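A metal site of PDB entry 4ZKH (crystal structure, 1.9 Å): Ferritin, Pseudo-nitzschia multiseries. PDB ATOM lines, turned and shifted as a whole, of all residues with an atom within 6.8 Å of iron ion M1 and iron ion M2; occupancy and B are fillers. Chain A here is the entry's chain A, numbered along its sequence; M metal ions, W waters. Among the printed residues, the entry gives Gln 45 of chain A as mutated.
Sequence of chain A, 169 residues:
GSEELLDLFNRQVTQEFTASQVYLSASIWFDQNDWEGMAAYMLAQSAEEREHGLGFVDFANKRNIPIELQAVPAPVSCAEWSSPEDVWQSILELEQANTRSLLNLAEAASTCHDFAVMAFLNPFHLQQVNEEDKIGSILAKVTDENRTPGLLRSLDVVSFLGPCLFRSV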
ATOM      1  N   GLN A  12      12.966   2.847 -18.408  1.00  0.00           N
ATOM      2  CA  GLN A  12      12.537   1.691 -19.272  1.00  0.00           C
ATOM      3  C   GLN A  12      13.705   1.237 -20.095  1.00  0.00           C
ATOM      4  O   GLN A  12      13.897   0.044 -20.303  1.00  0.00           O
ATOM      5  CB  GLN A  12      11.326   1.997 -20.130  1.00  0.00           C
ATOM      6  CG  GLN A  12      10.787   0.768 -20.873  1.00  0.00           C
ATOM      7  CD  GLN A  12      10.202  -0.216 -19.860  1.00  0.00           C
ATOM      8  OE1 GLN A  12       9.674   0.223 -18.837  1.00  0.00           O
ATOM      9  NE2 GLN A  12      10.331  -1.535 -20.102  1.00  0.00           N
ATOM     10  N   GLN A  15      15.813  -0.868 -17.954  1.00  0.00           N
ATOM     11  CA  GLN A  15      15.163  -2.172 -17.791  1.00  0.00           C
ATOM     12  C   GLN A  15      15.353  -3.104 -18.978  1.00  0.00           C
ATOM     13  O   GLN A  15      15.618  -4.257 -18.755  1.00  0.00           O
ATOM     14  CB  GLN A  15      13.685  -1.989 -17.479  1.00  0.00           C
ATOM     15  CG  GLN A  15      12.965  -3.295 -17.245  1.00  0.00           C
ATOM     16  CD  GLN A  15      13.435  -4.055 -15.999  1.00  0.00           C
ATOM     17  OE1 GLN A  15      13.834  -3.448 -14.997  1.00  0.00           O
ATOM     18  NE2 GLN A  15      13.416  -5.411 -16.072  1.00  0.00           N
ATOM     19  N   GLU A  16      15.243  -2.601 -20.207  1.00  0.00           N
ATOM     20  CA  GLU A  16      15.399  -3.447 -21.377  1.00  0.00           C
ATOM     21  C   GLU A  16      16.834  -3.880 -21.436  1.00  0.00           C
ATOM     22  O   GLU A  16      17.113  -5.059 -21.684  1.00  0.00           O
ATOM     23  CB  GLU A  16      15.003  -2.683 -22.636  1.00  0.00           C
ATOM     24  CG  GLU A  16      13.597  -2.207 -22.655  1.00  0.00           C
ATOM     25  CD  GLU A  16      12.559  -3.325 -22.738  1.00  0.00           C
ATOM     26  OE1 GLU A  16      12.963  -4.417 -23.099  1.00  0.00           O
ATOM     27  OE2 GLU A  16      11.352  -3.060 -22.382  1.00  0.00           O
ATOM     28  N   ALA A  19      17.480  -6.532 -18.852  1.00  0.00           N
ATOM     29  CA  ALA A  19      17.000  -7.785 -19.388  1.00  0.00           C
ATOM     30  C   ALA A  19      17.942  -8.377 -20.402  1.00  0.00           C
ATOM     31  O   ALA A  19      18.205  -9.603 -20.350  1.00  0.00           O
ATOM     32  CB  ALA A  19      15.567  -7.610 -19.940  1.00  0.00           C
ATOM     33  N   TYR A  23      19.535 -12.136 -19.920  1.00  0.00           N
ATOM     34  CA  TYR A  23      19.478 -13.172 -20.992  1.00  0.00           C
ATOM     35  C   TYR A  23      20.868 -13.651 -21.358  1.00  0.00           C
ATOM     36  O   TYR A  23      21.049 -14.845 -21.578  1.00  0.00           O
ATOM     37  CB  TYR A  23      18.680 -12.650 -22.219  1.00  0.00           C
ATOM     38  CG  TYR A  23      17.181 -12.844 -22.143  1.00  0.00           C
ATOM     39  CD1 TYR A  23      16.650 -14.111 -22.264  1.00  0.00           C
ATOM     40  CD2 TYR A  23      16.302 -11.792 -22.081  1.00  0.00           C
ATOM     41  CE1 TYR A  23      15.301 -14.316 -22.246  1.00  0.00           C
ATOM     42  CE2 TYR A  23      14.979 -11.959 -22.019  1.00  0.00           C
ATOM     43  CZ  TYR A  23      14.451 -13.245 -22.172  1.00  0.00           C
ATOM     44  OH  TYR A  23      13.109 -13.466 -22.129  1.00  0.00           O
ATOM     45  N   GLN A  45      17.244 -13.843 -27.447  1.00  0.00           N
ATOM     46  CA  GLN A  45      16.449 -12.951 -26.627  1.00  0.00           C
ATOM     47  C   GLN A  45      17.293 -11.753 -26.051  1.00  0.00           C
ATOM     48  O   GLN A  45      16.776 -10.671 -25.908  1.00  0.00           O
ATOM     49  CB  GLN A  45      15.824 -13.725 -25.468  1.00  0.00           C
ATOM     50  CG  GLN A  45      14.565 -14.451 -25.871  1.00  0.00           C
ATOM     51  CD  GLN A  45      13.546 -13.432 -26.321  1.00  0.00           C
ATOM     52  OE1 GLN A  45      13.231 -12.464 -25.609  1.00  0.00           O
ATOM     53  NE2 GLN A  45      13.130 -13.559 -27.545  1.00  0.00           N
ATOM     54  N   GLU A  48      17.171  -9.312 -28.747  1.00  0.00           N
ATOM     55  CA  GLU A  48      15.855  -8.705 -28.848  1.00  0.00           C
ATOM     56  C   GLU A  48      15.627  -7.611 -27.740  1.00  0.00           C
ATOM     57  O   GLU A  48      15.072  -6.563 -28.021  1.00  0.00           O
ATOM     58  CB  GLU A  48      14.790  -9.772 -28.786  1.00  0.00           C
ATOM     59  CG  GLU A  48      13.334  -9.333 -28.748  1.00  0.00           C
ATOM     60  CD  GLU A  48      12.793  -8.958 -30.137  1.00  0.00           C
ATOM     61  OE1 GLU A  48      13.512  -9.229 -31.158  1.00  0.00           O
ATOM     62  OE2 GLU A  48      11.639  -8.381 -30.181  1.00  0.00           O
ATOM     63  N   GLU A  49      16.014  -7.879 -26.492  1.00  0.00           N
ATOM     64  CA  GLU A  49      15.809  -6.895 -25.459  1.00  0.00           C
ATOM     65  C   GLU A  49      16.608  -5.662 -25.722  1.00  0.00           C
ATOM     66  O   GLU A  49      16.118  -4.523 -25.458  1.00  0.00           O
ATOM     67  CB  GLU A  49      16.202  -7.494 -24.084  1.00  0.00           C
ATOM     68  CG  GLU A  49      15.363  -8.649 -23.696  1.00  0.00           C
ATOM     69  CD  GLU A  49      13.973  -8.269 -23.323  1.00  0.00           C
ATOM     70  OE1 GLU A  49      13.587  -7.097 -23.391  1.00  0.00           O
ATOM     71  OE2 GLU A  49      13.305  -9.140 -22.822  1.00  0.00           O
ATOM     72  N   ARG A  50      17.829  -5.814 -26.256  1.00  0.00           N
ATOM     73  CA  ARG A  50      18.618  -4.657 -26.636  1.00  0.00           C
ATOM     74  C   ARG A  50      17.890  -3.880 -27.719  1.00  0.00           C
ATOM     75  O   ARG A  50      17.863  -2.664 -27.664  1.00  0.00           O
ATOM     76  CB  ARG A  50      20.036  -5.027 -27.092  1.00  0.00           C
ATOM     77  CG  ARG A  50      20.877  -3.868 -27.645  1.00  0.00           C
ATOM     78  CD  ARG A  50      22.409  -4.107 -27.509  1.00  0.00           C
ATOM     79  NE  ARG A  50      23.215  -2.876 -27.817  1.00  0.00           N
ATOM     80  CZ  ARG A  50      23.387  -2.571 -29.085  1.00  0.00           C
ATOM     81  NH1 ARG A  50      22.820  -3.364 -29.982  1.00  0.00           N
ATOM     82  NH2 ARG A  50      23.980  -1.492 -29.500  1.00  0.00           N
ATOM     83  N   HIS A  52      14.718  -3.673 -27.991  1.00  0.00           N
ATOM     84  CA  HIS A  52      13.647  -2.907 -27.373  1.00  0.00           C
ATOM     85  C   HIS A  52      14.203  -1.636 -26.743  1.00  0.00           C
ATOM     86  O   HIS A  52      13.599  -0.605 -26.868  1.00  0.00           O
ATOM     87  CB  HIS A  52      12.926  -3.646 -26.262  1.00  0.00           C
ATOM     88  CG  HIS A  52      12.238  -4.903 -26.741  1.00  0.00           C
ATOM     89  ND1 HIS A  52      11.873  -5.925 -25.872  1.00  0.00           N
ATOM     90  CD2 HIS A  52      11.931  -5.337 -27.996  1.00  0.00           C
ATOM     91  CE1 HIS A  52      11.330  -6.913 -26.573  1.00  0.00           C
ATOM     92  NE2 HIS A  52      11.367  -6.598 -27.859  1.00  0.00           N
ATOM     93  N   GLY A  53      15.320  -1.743 -26.041  1.00  0.00           N
ATOM     94  CA  GLY A  53      15.942  -0.549 -25.465  1.00  0.00           C
ATOM     95  C   GLY A  53      16.292   0.492 -26.494  1.00  0.00           C
ATOM     96  O   GLY A  53      16.041   1.699 -26.296  1.00  0.00           O
ATOM     97  N   LEU A  94      11.846 -12.044 -14.920  1.00  0.00           N
ATOM     98  CA  LEU A  94      12.403 -10.901 -15.699  1.00  0.00           C
ATOM     99  C   LEU A  94      11.357 -10.351 -16.678  1.00  0.00           C
ATOM    100  O   LEU A  94      11.118  -9.147 -16.750  1.00  0.00           O
ATOM    101  CB  LEU A  94      13.606 -11.385 -16.489  1.00  0.00           C
ATOM    102  CG  LEU A  94      14.309 -10.354 -17.379  1.00  0.00           C
ATOM    103  CD1 LEU A  94      14.955  -9.319 -16.454  1.00  0.00           C
ATOM    104  CD2 LEU A  94      15.322 -11.044 -18.278  1.00  0.00           C
ATOM    105  N   GLU A  95      10.678 -11.226 -17.436  1.00  0.00           N
ATOM    106  CA  GLU A  95       9.693 -10.757 -18.371  1.00  0.00           C
ATOM    107  C   GLU A  95       8.511 -10.130 -17.665  1.00  0.00           C
ATOM    108  O   GLU A  95       8.016  -9.086 -18.110  1.00  0.00           O
ATOM    109  CB  GLU A  95       9.238 -11.801 -19.384  1.00  0.00           C
ATOM    110  CG  GLU A  95      10.385 -12.173 -20.280  1.00  0.00           C
ATOM    111  CD  GLU A  95      10.758 -11.092 -21.310  1.00  0.00           C
ATOM    112  OE1 GLU A  95      10.170  -9.978 -21.291  1.00  0.00           O
ATOM    113  OE2 GLU A  95      11.666 -11.443 -22.107  1.00  0.00           O
ATOM    114  N   ASN A  98       9.573  -6.729 -16.844  1.00  0.00           N
ATOM    115  CA  ASN A  98       9.559  -5.871 -18.043  1.00  0.00           C
ATOM    116  C   ASN A  98       8.119  -5.361 -18.260  1.00  0.00           C
ATOM    117  O   ASN A  98       7.882  -4.185 -18.480  1.00  0.00           O
ATOM    118  CB  ASN A  98      10.051  -6.600 -19.303  1.00  0.00           C
ATOM    119  CG  ASN A  98      11.550  -6.809 -19.334  1.00  0.00           C
ATOM    120  OD1 ASN A  98      12.307  -6.260 -18.507  1.00  0.00           O
ATOM    121  ND2 ASN A  98      11.989  -7.601 -20.304  1.00  0.00           N
ATOM    122  N   LEU A 102       6.454  -1.491 -18.145  1.00  0.00           N
ATOM    123  CA  LEU A 102       5.752  -0.887 -19.277  1.00  0.00           C
ATOM    124  C   LEU A 102       4.372  -0.416 -18.880  1.00  0.00           C
ATOM    125  O   LEU A 102       3.920   0.599 -19.347  1.00  0.00           O
ATOM    126  CB  LEU A 102       5.597  -1.882 -20.450  1.00  0.00           C
ATOM    127  CG  LEU A 102       6.906  -2.146 -21.166  1.00  0.00           C
ATOM    128  CD1 LEU A 102       6.791  -3.408 -22.020  1.00  0.00           C
ATOM    129  CD2 LEU A 102       7.282  -1.011 -22.100  1.00  0.00           C
ATOM    130  N   PHE A 124       4.401  -2.852 -27.574  1.00  0.00           N
ATOM    131  CA  PHE A 124       5.234  -3.451 -26.561  1.00  0.00           C
ATOM    132  C   PHE A 124       4.313  -4.196 -25.572  1.00  0.00           C
ATOM    133  O   PHE A 124       4.705  -5.239 -25.080  1.00  0.00           O
ATOM    134  CB  PHE A 124       6.102  -2.407 -25.824  1.00  0.00           C
ATOM    135  CG  PHE A 124       7.204  -1.876 -26.689  1.00  0.00           C
ATOM    136  CD1 PHE A 124       8.419  -2.562 -26.794  1.00  0.00           C
ATOM    137  CD2 PHE A 124       7.012  -0.713 -27.451  1.00  0.00           C
ATOM    138  CE1 PHE A 124       9.424  -2.080 -27.615  1.00  0.00           C
ATOM    139  CE2 PHE A 124       8.019  -0.222 -28.289  1.00  0.00           C
ATOM    140  CZ  PHE A 124       9.236  -0.933 -28.394  1.00  0.00           C
ATOM    141  N   GLN A 127       3.467  -7.400 -27.397  1.00  0.00           N
ATOM    142  CA  GLN A 127       4.663  -8.264 -27.401  1.00  0.00           C
ATOM    143  C   GLN A 127       4.830  -8.950 -26.001  1.00  0.00           C
ATOM    144  O   GLN A 127       5.180 -10.110 -25.908  1.00  0.00           O
ATOM    145  CB  GLN A 127       5.860  -7.384 -27.736  1.00  0.00           C
ATOM    146  CG  GLN A 127       7.216  -8.069 -27.626  1.00  0.00           C
ATOM    147  CD  GLN A 127       7.537  -8.883 -28.832  1.00  0.00           C
ATOM    148  OE1 GLN A 127       6.681  -9.066 -29.744  1.00  0.00           O
ATOM    149  NE2 GLN A 127       8.762  -9.418 -28.871  1.00  0.00           N
ATOM    150  N   GLN A 128       4.742  -8.201 -24.940  1.00  0.00           N
ATOM    151  CA  GLN A 128       4.940  -8.813 -23.590  1.00  0.00           C
ATOM    152  C   GLN A 128       3.951  -9.952 -23.309  1.00  0.00           C
ATOM    153  O   GLN A 128       4.297 -10.910 -22.655  1.00  0.00           O
ATOM    154  CB  GLN A 128       4.815  -7.789 -22.507  1.00  0.00           C
ATOM    155  CG  GLN A 128       6.010  -6.877 -22.388  1.00  0.00           C
ATOM    156  CD  GLN A 128       7.359  -7.615 -22.440  1.00  0.00           C
ATOM    157  OE1 GLN A 128       8.128  -7.569 -23.443  1.00  0.00           O
ATOM    158  NE2 GLN A 128       7.662  -8.307 -21.343  1.00  0.00           N
ATOM    159  N   GLU A 131       5.342 -12.814 -25.134  1.00  0.00           N
ATOM    160  CA  GLU A 131       6.564 -13.297 -24.509  1.00  0.00           C
ATOM    161  C   GLU A 131       6.332 -14.034 -23.171  1.00  0.00           C
ATOM    162  O   GLU A 131       7.005 -15.073 -22.920  1.00  0.00           O
ATOM    163  CB  GLU A 131       7.584 -12.160 -24.317  1.00  0.00           C
ATOM    164  CG  GLU A 131       8.243 -11.706 -25.632  1.00  0.00           C
ATOM    165  CD  GLU A 131       9.289 -10.629 -25.389  1.00  0.00           C
ATOM    166  OE1 GLU A 131       9.636 -10.480 -24.205  1.00  0.00           O
ATOM    167  OE2 GLU A 131       9.726  -9.894 -26.327  1.00  0.00           O
HETATM  168 FE    FE M   1      11.828  -6.132 -23.490  1.00  0.00          FE
HETATM  169 FE    FE M   2      11.434  -9.604 -23.397  1.00  0.00          FE
HETATM  170  O   HOH W   1      12.471 -10.111 -25.303  1.00  0.00           O
HETATM  171  O   HOH W   2      10.673  -7.960 -23.321  1.00  0.00           O
HETATM  172  O   HOH W   3      10.062  -5.161 -23.238  1.00  0.00           O
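The side-chain carboxylate (OE1) of Glu 95 lies close to the side-chain amide nitrogen (ND2) of Asn 98, at 3.2 Å.
OE2 of Glu 49 sits close to ND2 of Asn 98, 3.2 Å away.
OD1 of Asn 98 is in hydrogen-bond range of NE2 of Gln 15, at 2.8 Å.
The side-chain hydroxyl (OH) of Tyr 23 sits close to the side-chain carboxylate (OE2) of Glu 95 (2.5 Å).
The side-chain carboxylate of Glu 131 is in hydrogen-bond range of the side-chain amide nitrogen of Gln 127.
NE2 of His 52 is in hydrogen-bond range of OE2 of Glu 48, 2.9 Å away.
The side-chain amide nitrogen (NE2) of Gln 12 sits at hydrogen-bond distance from the side-chain carboxylate (OE2) of Glu 16 (2.9 Å).
O of Glu 95 lies within hydrogen-bond range of NE2 of Gln 128 (3.3 Å).
Asn 98 touches iron ion M1 (ND2 to FE, 3.5 Å).
OE1 of Gln 128 touches iron ion M1, 3.97 Å away.
Of the 19 residues printed, 5 come within 4 Å of iron ion M1.
The nearest printed residue that does not touch iron ion M1 is Glu 95 (4.7 Å).
Asn 98 touches iron ion M2 (ND2 to FE, 3.7 Å).
Gln 128 touches iron ion M2 (OE1 to FE, 3.9 Å).
Of the 19 residues printed, 5 come within 4 Å of iron ion M2.
Iron ion M1 is bound by the side-chain carboxylate (OE1) of Glu 49 (2.0 Å), water W3 (2.0 Å), the side-chain carboxylate (OE1) of Glu 16 (2.1 Å), water W2 (2.2 Å) and a ring nitrogen (ND1) of His 52 (2.4 Å).
Iron ion M2 is bound by water W2 (1.8 Å), OE2 of Glu 49 (2.0 Å), OE1 of Glu 131 (2.2 Å), water W1 (2.2 Å), OE2 of Glu 95 (2.3 Å) and OE1 of Glu 95 (2.5 Å).
Water W2 bridges OE1 of Gln 128 (2.6 Å) and ND2 of Asn 98 (3.3 Å).
Water W3 bridges the side-chain carboxylate of Glu 16 (2.6 Å) and the side-chain amide oxygen of Gln 128 (3.1 Å).
Water W1 bridges the side-chain amide oxygen (OE1) of Gln 45 and the side-chain carboxylate (OE2) of Glu 131.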
